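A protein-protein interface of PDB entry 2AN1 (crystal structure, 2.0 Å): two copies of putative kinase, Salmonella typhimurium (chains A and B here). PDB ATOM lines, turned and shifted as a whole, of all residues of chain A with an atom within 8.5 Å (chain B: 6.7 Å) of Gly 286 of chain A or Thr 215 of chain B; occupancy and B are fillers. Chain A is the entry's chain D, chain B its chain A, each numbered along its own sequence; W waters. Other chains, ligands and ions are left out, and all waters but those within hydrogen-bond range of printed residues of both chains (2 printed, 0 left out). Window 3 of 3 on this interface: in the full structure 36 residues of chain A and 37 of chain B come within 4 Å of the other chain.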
ATOM      1  N   ASN A 279     -13.590  23.810   3.615  1.00  0.00           N
ATOM      2  CA  ASN A 279     -14.239  22.540   3.369  1.00  0.00           C
ATOM      3  C   ASN A 279     -13.255  21.385   3.588  1.00  0.00           C
ATOM      4  O   ASN A 279     -13.585  20.433   4.273  1.00  0.00           O
ATOM      5  CB  ASN A 279     -14.841  22.480   1.968  1.00  0.00           C
ATOM      6  CG  ASN A 279     -15.397  21.112   1.641  1.00  0.00           C
ATOM      7  OD1 ASN A 279     -16.429  20.697   2.173  1.00  0.00           O
ATOM      8  ND2 ASN A 279     -14.695  20.391   0.783  1.00  0.00           N
ATOM      9  N   THR A 280     -12.067  21.474   2.990  1.00  0.00           N
ATOM     10  CA  THR A 280     -11.018  20.474   3.209  1.00  0.00           C
ATOM     11  C   THR A 280     -10.668  20.301   4.709  1.00  0.00           C
ATOM     12  O   THR A 280     -10.628  19.163   5.219  1.00  0.00           O
ATOM     13  CB  THR A 280      -9.729  20.819   2.411  1.00  0.00           C
ATOM     14  OG1 THR A 280     -10.039  20.915   1.018  1.00  0.00           O
ATOM     15  CG2 THR A 280      -8.653  19.756   2.619  1.00  0.00           C
ATOM     16  N   LEU A 281     -10.421  21.419   5.399  1.00  0.00           N
ATOM     17  CA  LEU A 281     -10.058  21.395   6.823  1.00  0.00           C
ATOM     18  C   LEU A 281     -11.141  20.683   7.666  1.00  0.00           C
ATOM     19  O   LEU A 281     -10.873  19.726   8.409  1.00  0.00           O
ATOM     20  CB  LEU A 281      -9.846  22.827   7.334  1.00  0.00           C
ATOM     21  CG  LEU A 281      -9.417  23.030   8.792  1.00  0.00           C
ATOM     22  CD1 LEU A 281      -7.996  22.438   8.989  1.00  0.00           C
ATOM     23  CD2 LEU A 281      -9.449  24.520   9.171  1.00  0.00           C
ATOM     24  N   SER A 282     -12.368  21.156   7.524  1.00  0.00           N
ATOM     25  CA  SER A 282     -13.500  20.601   8.255  1.00  0.00           C
ATOM     26  C   SER A 282     -13.708  19.125   7.941  1.00  0.00           C
ATOM     27  O   SER A 282     -13.999  18.332   8.838  1.00  0.00           O
ATOM     28  CB  SER A 282     -14.764  21.403   7.950  1.00  0.00           C
ATOM     29  OG  SER A 282     -14.715  22.626   8.693  1.00  0.00           O
ATOM     30  N   THR A 283     -13.526  18.754   6.674  1.00  0.00           N
ATOM     31  CA  THR A 283     -13.725  17.371   6.256  1.00  0.00           C
ATOM     32  C   THR A 283     -12.635  16.464   6.855  1.00  0.00           C
ATOM     33  O   THR A 283     -12.935  15.420   7.408  1.00  0.00           O
ATOM     34  CB  THR A 283     -13.755  17.232   4.710  1.00  0.00           C
ATOM     35  OG1 THR A 283     -14.777  18.084   4.159  1.00  0.00           O
ATOM     36  CG2 THR A 283     -14.041  15.771   4.290  1.00  0.00           C
ATOM     37  N   LYS A 284     -11.378  16.873   6.740  1.00  0.00           N
ATOM     38  CA  LYS A 284     -10.266  16.063   7.254  1.00  0.00           C
ATOM     39  C   LYS A 284     -10.257  15.918   8.780  1.00  0.00           C
ATOM     40  O   LYS A 284      -9.906  14.871   9.293  1.00  0.00           O
ATOM     41  CB  LYS A 284      -8.940  16.612   6.748  1.00  0.00           C
ATOM     42  CG  LYS A 284      -8.722  16.299   5.262  1.00  0.00           C
ATOM     43  CD  LYS A 284      -7.297  16.571   4.810  1.00  0.00           C
ATOM     44  CE  LYS A 284      -6.327  15.510   5.350  1.00  0.00           C
ATOM     45  NZ  LYS A 284      -6.569  14.171   4.754  1.00  0.00           N
ATOM     46  N   LEU A 285     -10.676  16.965   9.492  1.00  0.00           N
ATOM     47  CA  LEU A 285     -10.656  16.976  10.963  1.00  0.00           C
ATOM     48  C   LEU A 285     -11.963  16.528  11.602  1.00  0.00           C
ATOM     49  O   LEU A 285     -12.061  16.454  12.828  1.00  0.00           O
ATOM     50  CB  LEU A 285     -10.275  18.371  11.487  1.00  0.00           C
ATOM     51  CG  LEU A 285      -8.771  18.665  11.550  1.00  0.00           C
ATOM     52  CD1 LEU A 285      -8.003  18.144  10.381  1.00  0.00           C
ATOM     53  CD2 LEU A 285      -8.410  20.129  11.811  1.00  0.00           C
ATOM     54  N   GLY A 286     -12.975  16.247  10.788  1.00  0.00           N
ATOM     55  CA  GLY A 286     -14.254  15.782  11.328  1.00  0.00           C
ATOM     56  C   GLY A 286     -15.088  16.858  12.013  1.00  0.00           C
ATOM     57  O   GLY A 286     -15.903  16.543  12.895  1.00  0.00           O
ATOM     58  N   TRP A 287     -14.890  18.122  11.619  1.00  0.00           N
ATOM     59  CA  TRP A 287     -15.682  19.239  12.130  1.00  0.00           C
ATOM     60  C   TRP A 287     -17.091  19.203  11.522  1.00  0.00           C
ATOM     61  O   TRP A 287     -17.270  18.727  10.394  1.00  0.00           O
ATOM     62  CB  TRP A 287     -14.994  20.575  11.805  1.00  0.00           C
ATOM     63  CG  TRP A 287     -13.698  20.800  12.532  1.00  0.00           C
ATOM     64  CD1 TRP A 287     -13.044  19.919  13.362  1.00  0.00           C
ATOM     65  CD2 TRP A 287     -12.871  21.962  12.461  1.00  0.00           C
ATOM     66  NE1 TRP A 287     -11.882  20.474  13.817  1.00  0.00           N
ATOM     67  CE2 TRP A 287     -11.740  21.722  13.274  1.00  0.00           C
ATOM     68  CE3 TRP A 287     -12.978  23.192  11.790  1.00  0.00           C
ATOM     69  CZ2 TRP A 287     -10.724  22.670  13.448  1.00  0.00           C
ATOM     70  CZ3 TRP A 287     -11.966  24.130  11.958  1.00  0.00           C
ATOM     71  CH2 TRP A 287     -10.859  23.866  12.788  1.00  0.00           C
ATOM     72  N   SER A 288     -18.087  19.684  12.264  1.00  0.00           N
ATOM     73  CA  SER A 288     -19.463  19.683  11.753  1.00  0.00           C
ATOM     74  C   SER A 288     -19.596  20.620  10.534  1.00  0.00           C
ATOM     75  O   SER A 288     -18.949  21.674  10.466  1.00  0.00           O
ATOM     76  CB  SER A 288     -20.461  20.028  12.857  1.00  0.00           C
ATOM     77  OG  SER A 288     -21.793  19.941  12.360  1.00  0.00           O
ATOM     78  N   LYS A 289     -20.348  20.167   9.537  1.00  0.00           N
ATOM     79  CA  LYS A 289     -20.609  20.941   8.325  1.00  0.00           C
ATOM     80  C   LYS A 289     -22.105  21.156   8.202  1.00  0.00           C
ATOM     81  O   LYS A 289     -22.619  21.421   7.125  1.00  0.00           O
ATOM     82  CB  LYS A 289     -19.997  20.273   7.077  1.00  0.00           C
ATOM     83  CG  LYS A 289     -18.434  20.234   7.119  1.00  0.00           C
ATOM     84  CD  LYS A 289     -17.779  19.840   5.765  1.00  0.00           C
ATOM     85  CE  LYS A 289     -18.155  18.420   5.339  1.00  0.00           C
ATOM     86  NZ  LYS A 289     -17.556  18.070   4.015  1.00  0.00           N
ATOM     87  N   SER B 173     -19.764  24.302  11.416  1.00  0.00           N
ATOM     88  CA  SER B 173     -20.740  24.549  12.467  1.00  0.00           C
ATOM     89  C   SER B 173     -20.176  24.040  13.775  1.00  0.00           C
ATOM     90  O   SER B 173     -19.314  23.166  13.777  1.00  0.00           O
ATOM     91  CB  SER B 173     -22.034  23.795  12.171  1.00  0.00           C
ATOM     92  OG  SER B 173     -22.717  24.484  11.156  1.00  0.00           O
ATOM     93  N   GLN B 174     -20.725  24.532  14.883  1.00  0.00           N
ATOM     94  CA  GLN B 174     -20.234  24.172  16.194  1.00  0.00           C
ATOM     95  C   GLN B 174     -21.392  24.146  17.198  1.00  0.00           C
ATOM     96  O   GLN B 174     -22.301  24.987  17.118  1.00  0.00           O
ATOM     97  CB  GLN B 174     -19.180  25.203  16.608  1.00  0.00           C
ATOM     98  CG  GLN B 174     -18.423  24.907  17.871  1.00  0.00           C
ATOM     99  CD  GLN B 174     -17.160  25.766  18.002  1.00  0.00           C
ATOM    100  OE1 GLN B 174     -16.245  25.676  17.169  1.00  0.00           O
ATOM    101  NE2 GLN B 174     -17.098  26.585  19.065  1.00  0.00           N
ATOM    102  N   ARG B 175     -21.380  23.150  18.091  1.00  0.00           N
ATOM    103  CA  ARG B 175     -22.178  23.184  19.331  1.00  0.00           C
ATOM    104  C   ARG B 175     -21.221  23.355  20.513  1.00  0.00           C
ATOM    105  O   ARG B 175     -20.359  22.505  20.729  1.00  0.00           O
ATOM    106  CB  ARG B 175     -23.000  21.900  19.515  1.00  0.00           C
ATOM    107  CG  ARG B 175     -23.928  21.569  18.354  1.00  0.00           C
ATOM    108  CD  ARG B 175     -24.787  20.324  18.635  1.00  0.00           C
ATOM    109  NE  ARG B 175     -24.086  19.106  18.219  1.00  0.00           N
ATOM    110  CZ  ARG B 175     -24.598  17.876  18.250  1.00  0.00           C
ATOM    111  NH1 ARG B 175     -25.836  17.666  18.699  1.00  0.00           N
ATOM    112  NH2 ARG B 175     -23.862  16.845  17.843  1.00  0.00           N
ATOM    113  N   PHE B 212     -15.413  25.162  24.882  1.00  0.00           N
ATOM    114  CA  PHE B 212     -15.944  23.832  25.184  1.00  0.00           C
ATOM    115  C   PHE B 212     -16.775  23.236  24.040  1.00  0.00           C
ATOM    116  O   PHE B 212     -17.963  22.952  24.202  1.00  0.00           O
ATOM    117  CB  PHE B 212     -16.754  23.843  26.494  1.00  0.00           C
ATOM    118  CG  PHE B 212     -15.992  24.369  27.701  1.00  0.00           C
ATOM    119  CD1 PHE B 212     -14.599  24.303  27.768  1.00  0.00           C
ATOM    120  CD2 PHE B 212     -16.679  24.904  28.778  1.00  0.00           C
ATOM    121  CE1 PHE B 212     -13.908  24.782  28.890  1.00  0.00           C
ATOM    122  CE2 PHE B 212     -15.996  25.390  29.906  1.00  0.00           C
ATOM    123  CZ  PHE B 212     -14.612  25.323  29.957  1.00  0.00           C
ATOM    124  N   PRO B 213     -16.154  23.047  22.873  1.00  0.00           N
ATOM    125  CA  PRO B 213     -16.932  22.503  21.777  1.00  0.00           C
ATOM    126  C   PRO B 213     -17.229  21.021  22.016  1.00  0.00           C
ATOM    127  O   PRO B 213     -16.417  20.299  22.633  1.00  0.00           O
ATOM    128  CB  PRO B 213     -16.006  22.684  20.584  1.00  0.00           C
ATOM    129  CG  PRO B 213     -14.635  22.600  21.181  1.00  0.00           C
ATOM    130  CD  PRO B 213     -14.748  23.284  22.496  1.00  0.00           C
ATOM    131  N   HIS B 214     -18.382  20.575  21.535  1.00  0.00           N
ATOM    132  CA  HIS B 214     -18.739  19.169  21.621  1.00  0.00           C
ATOM    133  C   HIS B 214     -17.848  18.286  20.734  1.00  0.00           C
ATOM    134  O   HIS B 214     -17.585  17.139  21.073  1.00  0.00           O
ATOM    135  CB  HIS B 214     -20.223  18.991  21.309  1.00  0.00           C
ATOM    136  CG  HIS B 214     -21.127  19.543  22.373  1.00  0.00           C
ATOM    137  ND1 HIS B 214     -20.862  20.721  23.046  1.00  0.00           N
ATOM    138  CD2 HIS B 214     -22.301  19.083  22.874  1.00  0.00           C
ATOM    139  CE1 HIS B 214     -21.832  20.959  23.911  1.00  0.00           C
ATOM    140  NE2 HIS B 214     -22.720  19.985  23.821  1.00  0.00           N
ATOM    141  N   THR B 215     -17.381  18.833  19.616  1.00  0.00           N
ATOM    142  CA  THR B 215     -16.439  18.135  18.735  1.00  0.00           C
ATOM    143  C   THR B 215     -15.024  18.185  19.320  1.00  0.00           C
ATOM    144  O   THR B 215     -14.421  19.259  19.433  1.00  0.00           O
ATOM    145  CB  THR B 215     -16.435  18.764  17.322  1.00  0.00           C
ATOM    146  OG1 THR B 215     -17.768  18.760  16.809  1.00  0.00           O
ATOM    147  CG2 THR B 215     -15.537  17.962  16.362  1.00  0.00           C
ATOM    148  N   LEU B 216     -14.500  17.014  19.670  1.00  0.00           N
ATOM    149  CA  LEU B 216     -13.211  16.894  20.365  1.00  0.00           C
ATOM    150  C   LEU B 216     -12.015  17.201  19.471  1.00  0.00           C
ATOM    151  O   LEU B 216     -10.924  17.466  19.971  1.00  0.00           O
ATOM    152  CB  LEU B 216     -13.068  15.510  21.008  1.00  0.00           C
ATOM    153  CG  LEU B 216     -14.212  15.083  21.951  1.00  0.00           C
ATOM    154  CD1 LEU B 216     -14.070  13.643  22.392  1.00  0.00           C
ATOM    155  CD2 LEU B 216     -14.340  16.003  23.158  1.00  0.00           C
ATOM    156  N   SER B 217     -12.224  17.186  18.155  1.00  0.00           N
ATOM    157  CA  SER B 217     -11.166  17.567  17.211  1.00  0.00           C
ATOM    158  C   SER B 217     -11.150  19.069  16.861  1.00  0.00           C
ATOM    159  O   SER B 217     -10.330  19.518  16.054  1.00  0.00           O
ATOM    160  CB  SER B 217     -11.280  16.730  15.931  1.00  0.00           C
ATOM    161  OG  SER B 217     -12.554  16.939  15.359  1.00  0.00           O
ATOM    162  N   ALA B 218     -12.047  19.845  17.460  1.00  0.00           N
ATOM    163  CA  ALA B 218     -12.006  21.304  17.307  1.00  0.00           C
ATOM    164  C   ALA B 218     -10.702  21.844  17.882  1.00  0.00           C
ATOM    165  O   ALA B 218     -10.242  21.379  18.924  1.00  0.00           O
ATOM    166  CB  ALA B 218     -13.197  21.963  17.999  1.00  0.00           C
ATOM    167  N   ARG B 219     -10.076  22.776  17.173  1.00  0.00           N
ATOM    168  CA  ARG B 219      -8.828  23.400  17.630  1.00  0.00           C
ATOM    169  C   ARG B 219      -8.876  24.885  17.286  1.00  0.00           C
ATOM    170  O   ARG B 219      -9.593  25.274  16.356  1.00  0.00           O
ATOM    171  CB  ARG B 219      -7.587  22.770  16.959  1.00  0.00           C
ATOM    172  CG  ARG B 219      -7.279  21.308  17.334  1.00  0.00           C
ATOM    173  CD  ARG B 219      -6.950  21.144  18.837  1.00  0.00           C
ATOM    174  NE  ARG B 219      -6.489  19.788  19.153  1.00  0.00           N
ATOM    175  CZ  ARG B 219      -7.275  18.728  19.380  1.00  0.00           C
ATOM    176  NH1 ARG B 219      -8.609  18.823  19.329  1.00  0.00           N
ATOM    177  NH2 ARG B 219      -6.711  17.555  19.682  1.00  0.00           N
HETATM  178  O   HOH W   1     -17.693  21.157  14.731  1.00  0.00           O
HETATM  179  O   HOH W   2     -18.464  16.907  13.927  1.00  0.00           O
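The backbone NH of Ser 173 of chain B lies within hydrogen-bond range of the backbone carbonyl oxygen of Ser 288 of chain A, at 2.9 Å. The backbone carbonyl oxygen (O) of Leu 285 of chain A lies within hydrogen-bond range of the side-chain hydroxyl (OG) of Ser 217 of chain B (2.6 Å). O of Ser 217 of chain B lies within hydrogen-bond range of NE1 of Trp 287 of chain A (2.9 Å).
Of chain B, only Thr 215 comes within 4 Å of Gly 286 of chain A. Of the printed residues of chain A, Ser 173 of chain B touches Ser 288. Printed residues of chain A within 4 Å of Ala 218 of chain B: Trp 287. Of the printed residues of chain B, Ser 288 of chain A touches Ser 173 (2.9 Å). Of the printed residues of chain B, Trp 287 of chain A touches Ser 217, Ala 218 and Arg 219. Of the printed residues of chain A, Ser 217 of chain B touches Leu 285 (2.6 Å) and Trp 287 (2.9 Å). Phe 212 of chain B touches none of the printed residues of chain A. The nearest residue of chain B that does not touch Gly 286 of chain A is Ser 217 of chain B (4.2 Å). The nearest printed residue of chain A that does not touch Ser 173 of chain B is Lys 289 of chain A (4.5 Å).
Among the printed residues, pairs that only touch across the chains: Trp 287 of chain A with Ala 218 of chain B (3.6 Å), Gly 286 of chain A with Thr 215 of chain B (3.8 Å) and Trp 287 of chain A with Arg 219 of chain B (3.8 Å).
Among the printed residues, 6 pairs touch across the chains. Among the printed residues, no Asp or Glu carboxylate lies within 4 Å of a Lys or Arg side-chain nitrogen of the other chain.
Water W1 lies within hydrogen-bond range of the backbone carbonyl oxygen of Ser 173 of chain B (2.8 Å), the backbone NH of Ser 288 of chain A (2.9 Å) and the side-chain hydroxyl of Thr 215 of chain B (3.2 Å). Water W2 lies within hydrogen-bond range of the backbone carbonyl oxygen of Gly 286 of chain A (2.8 Å), the backbone NH of Ser 288 of chain A (3.3 Å) and the side-chain hydroxyl of Thr 215 of chain B (3.5 Å).
The backbone carbonyl oxygen of Leu 216 of chain B sits at hydrogen-bond distance from the guanidinium group of Arg 219 of chain B, at 2.8 Å. O of Ser 282 of chain A is in hydrogen-bond range of N of Trp 287 of chain A (2.9 Å).
No position is printed for both chains. Of the 6 pairs that touch across the chains among the printed residues, none has its exchanged pair printed and touching as well.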
